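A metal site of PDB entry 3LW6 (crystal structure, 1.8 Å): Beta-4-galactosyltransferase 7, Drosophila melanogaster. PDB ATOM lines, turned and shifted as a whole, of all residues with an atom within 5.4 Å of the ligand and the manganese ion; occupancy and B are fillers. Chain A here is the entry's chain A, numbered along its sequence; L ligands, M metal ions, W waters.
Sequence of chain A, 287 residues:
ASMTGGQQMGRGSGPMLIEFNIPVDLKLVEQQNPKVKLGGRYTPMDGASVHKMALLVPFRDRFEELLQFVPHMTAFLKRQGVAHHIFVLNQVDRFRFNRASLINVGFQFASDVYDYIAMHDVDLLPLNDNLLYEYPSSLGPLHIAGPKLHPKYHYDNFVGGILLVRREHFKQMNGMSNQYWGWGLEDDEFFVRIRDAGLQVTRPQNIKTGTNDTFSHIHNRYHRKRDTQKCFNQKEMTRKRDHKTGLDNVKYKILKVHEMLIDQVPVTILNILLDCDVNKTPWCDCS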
ATOM      1  N   VAL A  57      12.632   0.395  17.602  1.00  0.00           N
ATOM      2  CA  VAL A  57      11.345   0.769  18.180  1.00  0.00           C
ATOM      3  C   VAL A  57      10.625  -0.505  18.624  1.00  0.00           C
ATOM      4  O   VAL A  57      10.067  -1.243  17.803  1.00  0.00           O
ATOM      5  CB  VAL A  57      10.465   1.517  17.160  1.00  0.00           C
ATOM      6  CG1 VAL A  57       9.189   1.993  17.837  1.00  0.00           C
ATOM      7  CG2 VAL A  57      11.216   2.763  16.601  1.00  0.00           C
ATOM      8  N   PRO A  58      10.634  -0.788  19.907  1.00  0.00           N
ATOM      9  CA  PRO A  58       9.881  -1.929  20.479  1.00  0.00           C
ATOM     10  C   PRO A  58       8.408  -1.729  20.166  1.00  0.00           C
ATOM     11  O   PRO A  58       7.917  -0.580  20.219  1.00  0.00           O
ATOM     12  CB  PRO A  58      10.199  -1.882  21.969  1.00  0.00           C
ATOM     13  CG  PRO A  58      10.839  -0.561  22.175  1.00  0.00           C
ATOM     14  CD  PRO A  58      11.249   0.083  20.933  1.00  0.00           C
ATOM     15  N   PHE A  59       7.732  -2.804  19.728  1.00  0.00           N
ATOM     16  CA  PHE A  59       6.406  -2.615  19.118  1.00  0.00           C
ATOM     17  C   PHE A  59       5.522  -3.823  19.296  1.00  0.00           C
ATOM     18  O   PHE A  59       5.916  -4.948  18.950  1.00  0.00           O
ATOM     19  CB  PHE A  59       6.547  -2.319  17.611  1.00  0.00           C
ATOM     20  CG  PHE A  59       5.199  -2.011  16.926  1.00  0.00           C
ATOM     21  CD1 PHE A  59       4.812  -0.693  16.713  1.00  0.00           C
ATOM     22  CD2 PHE A  59       4.391  -3.051  16.474  1.00  0.00           C
ATOM     23  CE1 PHE A  59       3.611  -0.436  16.037  1.00  0.00           C
ATOM     24  CE2 PHE A  59       3.123  -2.803  15.861  1.00  0.00           C
ATOM     25  CZ  PHE A  59       2.766  -1.489  15.652  1.00  0.00           C
ATOM     26  N   ARG A  60       4.289  -3.557  19.772  1.00  0.00           N
ATOM     27  CA  ARG A  60       3.216  -4.529  19.640  1.00  0.00           C
ATOM     28  C   ARG A  60       1.919  -3.736  19.827  1.00  0.00           C
ATOM     29  O   ARG A  60       1.752  -3.012  20.872  1.00  0.00           O
ATOM     30  CB  ARG A  60       3.280  -5.549  20.740  1.00  0.00           C
ATOM     31  CG  ARG A  60       2.075  -6.507  20.676  1.00  0.00           C
ATOM     32  CD  ARG A  60       2.018  -7.214  22.017  1.00  0.00           C
ATOM     33  NE  ARG A  60       2.777  -8.425  21.835  1.00  0.00           N
ATOM     34  CZ  ARG A  60       3.129  -9.267  22.787  1.00  0.00           C
ATOM     35  NH1 ARG A  60       2.881  -9.044  24.095  1.00  0.00           N
ATOM     36  NH2 ARG A  60       3.760 -10.374  22.391  1.00  0.00           N
ATOM     37  N   ASP A  61       1.036  -3.899  18.847  1.00  0.00           N
ATOM     38  CA  ASP A  61      -0.285  -3.196  18.859  1.00  0.00           C
ATOM     39  C   ASP A  61      -0.177  -1.645  19.062  1.00  0.00           C
ATOM     40  O   ASP A  61      -0.864  -1.103  19.936  1.00  0.00           O
ATOM     41  CB  ASP A  61      -1.088  -3.737  20.099  1.00  0.00           C
ATOM     42  CG  ASP A  61      -1.444  -5.251  19.962  1.00  0.00           C
ATOM     43  OD1 ASP A  61      -1.333  -5.794  18.844  1.00  0.00           O
ATOM     44  OD2 ASP A  61      -1.767  -5.883  20.990  1.00  0.00           O
ATOM     45  N   ARG A  62       0.640  -0.960  18.278  1.00  0.00           N
ATOM     46  CA  ARG A  62       0.824   0.495  18.435  1.00  0.00           C
ATOM     47  C   ARG A  62       0.801   1.117  17.054  1.00  0.00           C
ATOM     48  O   ARG A  62       1.493   2.103  16.774  1.00  0.00           O
ATOM     49  CB  ARG A  62       2.146   0.833  19.177  1.00  0.00           C
ATOM     50  CG  ARG A  62       2.161   0.330  20.604  1.00  0.00           C
ATOM     51  CD  ARG A  62       1.189   1.092  21.563  1.00  0.00           C
ATOM     52  NE  ARG A  62       1.330   0.695  22.985  1.00  0.00           N
ATOM     53  CZ  ARG A  62       0.731  -0.365  23.518  1.00  0.00           C
ATOM     54  NH1 ARG A  62      -0.087  -1.161  22.779  1.00  0.00           N
ATOM     55  NH2 ARG A  62       0.925  -0.656  24.793  1.00  0.00           N
ATOM     56  N   PHE A  97       4.946  -8.539  26.858  1.00  0.00           N
ATOM     57  CA  PHE A  97       5.805  -7.683  26.078  1.00  0.00           C
ATOM     58  C   PHE A  97       7.208  -7.598  26.731  1.00  0.00           C
ATOM     59  O   PHE A  97       7.323  -7.297  27.933  1.00  0.00           O
ATOM     60  CB  PHE A  97       5.176  -6.286  25.979  1.00  0.00           C
ATOM     61  CG  PHE A  97       5.848  -5.417  24.939  1.00  0.00           C
ATOM     62  CD1 PHE A  97       5.707  -5.684  23.596  1.00  0.00           C
ATOM     63  CD2 PHE A  97       6.691  -4.399  25.345  1.00  0.00           C
ATOM     64  CE1 PHE A  97       6.344  -4.880  22.593  1.00  0.00           C
ATOM     65  CE2 PHE A  97       7.330  -3.599  24.384  1.00  0.00           C
ATOM     66  CZ  PHE A  97       7.172  -3.846  23.005  1.00  0.00           C
ATOM     67  N   ARG A  99      10.340  -5.517  26.074  1.00  0.00           N
ATOM     68  CA  ARG A  99      11.037  -4.438  25.424  1.00  0.00           C
ATOM     69  C   ARG A  99      12.537  -4.702  25.260  1.00  0.00           C
ATOM     70  O   ARG A  99      13.106  -4.475  24.157  1.00  0.00           O
ATOM     71  CB  ARG A  99      10.866  -3.146  26.295  1.00  0.00           C
ATOM     72  CG  ARG A  99      11.527  -1.891  25.669  1.00  0.00           C
ATOM     73  CD  ARG A  99      11.124  -0.643  26.527  1.00  0.00           C
ATOM     74  NE  ARG A  99      11.743   0.587  25.988  1.00  0.00           N
ATOM     75  CZ  ARG A  99      12.890   1.112  26.453  1.00  0.00           C
ATOM     76  NH1 ARG A  99      13.548   0.535  27.460  1.00  0.00           N
ATOM     77  NH2 ARG A  99      13.338   2.255  25.902  1.00  0.00           N
ATOM     78  N   HIS A 120      14.055   3.354  21.269  1.00  0.00           N
ATOM     79  CA  HIS A 120      13.166   4.498  21.197  1.00  0.00           C
ATOM     80  C   HIS A 120      11.679   4.059  21.362  1.00  0.00           C
ATOM     81  O   HIS A 120      11.158   3.354  20.512  1.00  0.00           O
ATOM     82  CB  HIS A 120      13.307   5.195  19.829  1.00  0.00           C
ATOM     83  CG  HIS A 120      12.887   6.646  19.865  1.00  0.00           C
ATOM     84  ND1 HIS A 120      13.696   7.691  19.480  1.00  0.00           N
ATOM     85  CD2 HIS A 120      11.717   7.205  20.285  1.00  0.00           C
ATOM     86  CE1 HIS A 120      13.057   8.849  19.691  1.00  0.00           C
ATOM     87  NE2 HIS A 120      11.836   8.567  20.146  1.00  0.00           N
ATOM     88  N   ASP A 121      11.025   4.506  22.412  1.00  0.00           N
ATOM     89  CA  ASP A 121       9.583   4.244  22.528  1.00  0.00           C
ATOM     90  C   ASP A 121       8.828   4.848  21.383  1.00  0.00           C
ATOM     91  O   ASP A 121       9.116   5.955  20.954  1.00  0.00           O
ATOM     92  CB  ASP A 121       9.057   4.724  23.871  1.00  0.00           C
ATOM     93  CG  ASP A 121       9.669   3.908  25.056  1.00  0.00           C
ATOM     94  OD1 ASP A 121      10.445   2.958  24.818  1.00  0.00           O
ATOM     95  OD2 ASP A 121       9.377   4.271  26.196  1.00  0.00           O
ATOM     96  N   VAL A 122       7.762   4.165  20.953  1.00  0.00           N
ATOM     97  CA  VAL A 122       7.058   4.626  19.727  1.00  0.00           C
ATOM     98  C   VAL A 122       6.136   5.833  20.039  1.00  0.00           C
ATOM     99  O   VAL A 122       5.648   6.467  19.116  1.00  0.00           O
ATOM    100  CB  VAL A 122       6.218   3.469  19.160  1.00  0.00           C
ATOM    101  CG1 VAL A 122       5.050   3.171  20.126  1.00  0.00           C
ATOM    102  CG2 VAL A 122       5.778   3.722  17.744  1.00  0.00           C
ATOM    103  N   ASP A 123       5.903   6.109  21.330  1.00  0.00           N
ATOM    104  CA  ASP A 123       4.858   7.078  21.725  1.00  0.00           C
ATOM    105  C   ASP A 123       5.481   8.359  22.302  1.00  0.00           C
ATOM    106  O   ASP A 123       4.793   9.185  22.874  1.00  0.00           O
ATOM    107  CB  ASP A 123       3.857   6.469  22.766  1.00  0.00           C
ATOM    108  CG  ASP A 123       4.538   6.074  24.057  1.00  0.00           C
ATOM    109  OD1 ASP A 123       5.779   6.310  24.128  1.00  0.00           O
ATOM    110  OD2 ASP A 123       3.942   5.488  25.012  1.00  0.00           O
ATOM    111  N   HIS A 150      11.512  14.318  30.792  1.00  0.00           N
ATOM    112  CA  HIS A 150      10.430  13.363  30.635  1.00  0.00           C
ATOM    113  C   HIS A 150       9.134  13.776  31.366  1.00  0.00           C
ATOM    114  O   HIS A 150       9.157  14.199  32.525  1.00  0.00           O
ATOM    115  CB  HIS A 150      10.896  11.980  31.130  1.00  0.00           C
ATOM    116  CG  HIS A 150       9.975  10.871  30.707  1.00  0.00           C
ATOM    117  ND1 HIS A 150      10.270   9.996  29.683  1.00  0.00           N
ATOM    118  CD2 HIS A 150       8.736  10.539  31.140  1.00  0.00           C
ATOM    119  CE1 HIS A 150       9.263   9.148  29.529  1.00  0.00           C
ATOM    120  NE2 HIS A 150       8.321   9.448  30.411  1.00  0.00           N
ATOM    121  N   LYS A 152       6.814  12.075  32.729  1.00  0.00           N
ATOM    122  CA  LYS A 152       6.278  11.198  33.769  1.00  0.00           C
ATOM    123  C   LYS A 152       7.310  10.720  34.754  1.00  0.00           C
ATOM    124  O   LYS A 152       7.037  10.597  35.959  1.00  0.00           O
ATOM    125  CB  LYS A 152       5.597  10.005  33.058  1.00  0.00           C
ATOM    126  CG  LYS A 152       4.723   9.206  33.921  1.00  0.00           C
ATOM    127  CD  LYS A 152       4.053   8.077  33.128  1.00  0.00           C
ATOM    128  CE  LYS A 152       3.374   7.172  34.113  1.00  0.00           C
ATOM    129  NZ  LYS A 152       2.115   7.862  34.559  1.00  0.00           N
ATOM    130  N   TYR A 153       8.501  10.370  34.265  1.00  0.00           N
ATOM    131  CA  TYR A 153       9.509   9.772  35.130  1.00  0.00           C
ATOM    132  C   TYR A 153      10.653  10.712  35.460  1.00  0.00           C
ATOM    133  O   TYR A 153      11.302  11.210  34.564  1.00  0.00           O
ATOM    134  CB  TYR A 153      10.058   8.461  34.498  1.00  0.00           C
ATOM    135  CG  TYR A 153       8.939   7.495  34.181  1.00  0.00           C
ATOM    136  CD1 TYR A 153       8.093   7.038  35.188  1.00  0.00           C
ATOM    137  CD2 TYR A 153       8.718   7.034  32.874  1.00  0.00           C
ATOM    138  CE1 TYR A 153       7.045   6.170  34.910  1.00  0.00           C
ATOM    139  CE2 TYR A 153       7.653   6.178  32.566  1.00  0.00           C
ATOM    140  CZ  TYR A 153       6.856   5.698  33.631  1.00  0.00           C
ATOM    141  OH  TYR A 153       5.782   4.862  33.333  1.00  0.00           O
ATOM    142  N   TRP A 183       5.821  -4.817  31.921  1.00  0.00           N
ATOM    143  CA  TRP A 183       6.357  -3.469  32.205  1.00  0.00           C
ATOM    144  C   TRP A 183       7.309  -3.478  33.390  1.00  0.00           C
ATOM    145  O   TRP A 183       7.107  -4.197  34.421  1.00  0.00           O
ATOM    146  CB  TRP A 183       5.185  -2.511  32.486  1.00  0.00           C
ATOM    147  CG  TRP A 183       5.587  -1.093  32.658  1.00  0.00           C
ATOM    148  CD1 TRP A 183       5.572  -0.123  31.706  1.00  0.00           C
ATOM    149  CD2 TRP A 183       6.059  -0.495  33.852  1.00  0.00           C
ATOM    150  NE1 TRP A 183       5.986   1.085  32.249  1.00  0.00           N
ATOM    151  CE2 TRP A 183       6.324   0.874  33.561  1.00  0.00           C
ATOM    152  CE3 TRP A 183       6.292  -0.973  35.150  1.00  0.00           C
ATOM    153  CZ2 TRP A 183       6.827   1.774  34.531  1.00  0.00           C
ATOM    154  CZ3 TRP A 183       6.768  -0.091  36.135  1.00  0.00           C
ATOM    155  CH2 TRP A 183       7.038   1.287  35.807  1.00  0.00           C
ATOM    156  N   HIS A 217       4.020  12.802  24.910  1.00  0.00           N
ATOM    157  CA  HIS A 217       3.913  11.376  25.263  1.00  0.00           C
ATOM    158  C   HIS A 217       2.481  11.070  25.127  1.00  0.00           C
ATOM    159  O   HIS A 217       1.743  11.207  26.080  1.00  0.00           O
ATOM    160  CB  HIS A 217       4.395  11.145  26.698  1.00  0.00           C
ATOM    161  CG  HIS A 217       4.389   9.684  27.149  1.00  0.00           C
ATOM    162  ND1 HIS A 217       4.213   9.342  28.471  1.00  0.00           N
ATOM    163  CD2 HIS A 217       4.532   8.516  26.470  1.00  0.00           C
ATOM    164  CE1 HIS A 217       4.290   8.015  28.602  1.00  0.00           C
ATOM    165  NE2 HIS A 217       4.465   7.496  27.408  1.00  0.00           N
ATOM    166  N   HIS A 219      -0.010   8.848  25.442  1.00  0.00           N
ATOM    167  CA  HIS A 219      -0.149   7.480  25.960  1.00  0.00           C
ATOM    168  C   HIS A 219      -1.118   7.604  27.088  1.00  0.00           C
ATOM    169  O   HIS A 219      -0.767   8.084  28.213  1.00  0.00           O
ATOM    170  CB  HIS A 219       1.215   6.973  26.490  1.00  0.00           C
ATOM    171  CG  HIS A 219       1.177   5.617  27.158  1.00  0.00           C
ATOM    172  ND1 HIS A 219       2.339   4.899  27.446  1.00  0.00           N
ATOM    173  CD2 HIS A 219       0.142   4.821  27.575  1.00  0.00           C
ATOM    174  CE1 HIS A 219       2.022   3.747  28.027  1.00  0.00           C
ATOM    175  NE2 HIS A 219       0.697   3.671  28.124  1.00  0.00           N
ATOM    176  N   ARG A 226      -0.474  -0.609  30.947  1.00  0.00           N
ATOM    177  CA  ARG A 226       0.875  -1.088  31.265  1.00  0.00           C
ATOM    178  C   ARG A 226       0.714  -2.407  31.965  1.00  0.00           C
ATOM    179  O   ARG A 226      -0.070  -2.536  32.941  1.00  0.00           O
ATOM    180  CB  ARG A 226       1.603  -0.108  32.199  1.00  0.00           C
ATOM    181  CG  ARG A 226       1.935   1.193  31.480  1.00  0.00           C
ATOM    182  CD  ARG A 226       2.671   2.170  32.425  1.00  0.00           C
ATOM    183  NE  ARG A 226       3.012   3.415  31.672  1.00  0.00           N
ATOM    184  CZ  ARG A 226       2.217   4.461  31.471  1.00  0.00           C
ATOM    185  NH1 ARG A 226       0.947   4.501  31.937  1.00  0.00           N
ATOM    186  NH2 ARG A 226       2.686   5.485  30.734  1.00  0.00           N
HETATM  187  N1  LIG L   1       5.263  -1.145  23.802  1.00  0.00           N
HETATM  188  C1  LIG L   1       4.478  -1.632  22.786  1.00  0.00           C
HETATM  189  N2  LIG L   1       3.413  -2.483  23.083  1.00  0.00           N
HETATM  190  C2  LIG L   1       3.171  -2.811  24.400  1.00  0.00           C
HETATM  191  C3  LIG L   1       3.985  -2.310  25.459  1.00  0.00           C
HETATM  192  C4  LIG L   1       4.997  -1.340  25.154  1.00  0.00           C
HETATM  193  O1  LIG L   1       4.677  -1.369  21.599  1.00  0.00           O
HETATM  194  O2  LIG L   1       2.204  -3.635  24.590  1.00  0.00           O
HETATM  195  C5  LIG L   1       6.487  -0.300  23.411  1.00  0.00           C
HETATM  196  C6  LIG L   1       6.125   1.056  22.838  1.00  0.00           C
HETATM  197  O3  LIG L   1       7.167   1.460  21.937  1.00  0.00           O
HETATM  198  C7  LIG L   1       6.065   1.864  24.130  1.00  0.00           C
HETATM  199  C8  LIG L   1       7.324   1.284  24.823  1.00  0.00           C
HETATM  200  O4  LIG L   1       7.246  -0.142  24.589  1.00  0.00           O
HETATM  201  O5  LIG L   1       6.113   3.270  23.839  1.00  0.00           O
HETATM  202  C9  LIG L   1       7.445   1.548  26.319  1.00  0.00           C
HETATM  203  O6  LIG L   1       6.230   1.062  26.922  1.00  0.00           O
HETATM  204  P1  LIG L   1       5.230   2.098  27.709  1.00  0.00           P
HETATM  205  O7  LIG L   1       4.765   3.096  26.771  1.00  0.00           O
HETATM  206  O8  LIG L   1       4.107   1.305  28.328  1.00  0.00           O
HETATM  207  O9  LIG L   1       6.189   2.708  28.855  1.00  0.00           O
HETATM  208  P2  LIG L   1       6.051   4.084  29.710  1.00  0.00           P
HETATM  209  O10 LIG L   1       5.032   4.960  28.951  1.00  0.00           O
HETATM  210  O11 LIG L   1       5.748   3.680  31.073  1.00  0.00           O
HETATM  211  O12 LIG L   1       7.400   4.633  29.540  1.00  0.00           O
HETATM  212 MN    MN M   1       4.515   5.265  27.040  1.00  0.00          MN
HETATM  213  O   HOH W   1       8.306   6.842  28.364  1.00  0.00           O
HETATM  214  O   HOH W   2       7.432  -1.984  27.852  1.00  0.00           O
HETATM  215  O   HOH W   3       1.908  -4.754  27.275  1.00  0.00           O
HETATM  216  O   HOH W   4       6.724   5.517  26.404  1.00  0.00           O
HETATM  217  O   HOH W   5       2.439   1.850  25.224  1.00  0.00           O
HETATM  218  O   HOH W   6       1.687   0.171  27.768  1.00  0.00           O
HETATM  219  O   HOH W   7       4.901  -1.396  28.633  1.00  0.00           O
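CA of Phe 59 touches O1 of the ligand, at 3.3 Å.
CE2 of Phe 97 touches N1 of the ligand, at 3.3 Å.
CB of Asp 121 touches O5 of the ligand, at 3.3 Å.
Hydrophobic or aromatic side chains that line the ligand: Phe 97, Val 122, Tyr 153, Trp 183, His 217 and His 219.
Along chain A the residues within 4 Å of the ligand span positions 58 to 226.
The nearest printed residue that does not touch the ligand is Arg 99 (4.3 Å).
NE of Arg 99 is in salt-bridge range of OD1 of Asp 121, 2.9 Å away.
NH2 of Arg 226 sits close to ND1 of His 219, at 3.4 Å.
The backbone carbonyl oxygen (O) of Arg 60 sits at hydrogen-bond distance from the guanidinium group (NH1) of Arg 62 (3.2 Å).
Of the 19 residues printed, 3 come within 4 Å of the manganese ion.
The nearest printed residue that does not touch the manganese ion is Arg 226 (4.1 Å).
The manganese ion is bound by O10 of the ligand (2.0 Å), OD2 of Asp 123 (2.1 Å), O7 of the ligand (2.2 Å), ND1 of His 219 (2.2 Å), NE2 of His 217 (2.3 Å) and water W4 (2.3 Å).
Water W4 lies within hydrogen-bond range of OD1 of Asp 123 (2.6 Å), OD2 of Asp 121 (2.9 Å) and O12 of the ligand (3.3 Å).
Water W1 bridges O12 of the ligand (2.7 Å) and NE2 of His 150 (3.3 Å).
Water W6 bridges an oxygen (O8) of the ligand (2.7 Å) and the guanidinium group of Arg 62 (3.2 Å).
The guanidinium group of Arg 62 sits close to an oxygen (O2) of the ligand, 3.2 Å away.
O of Arg 60 is in hydrogen-bond range of N2 of the ligand (2.8 Å).
O of Pro 58 is in hydrogen-bond range of O3 of the ligand, 2.8 Å away.
The backbone NH (N) of Arg 60 is in hydrogen-bond range of an oxygen (O1) of the ligand (2.9 Å).
The backbone NH (N) of Val 122 sits at hydrogen-bond distance from an oxygen (O3) of the ligand (2.9 Å).
The side-chain hydroxyl of Tyr 153 is in hydrogen-bond range of an oxygen (O11) of the ligand (2.6 Å).
NE of Arg 226 lies within salt-bridge range of O11 of the ligand (2.8 Å).
The indole nitrogen (NE1) of Trp 183 sits at hydrogen-bond distance from an oxygen (O11) of the ligand (2.9 Å).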
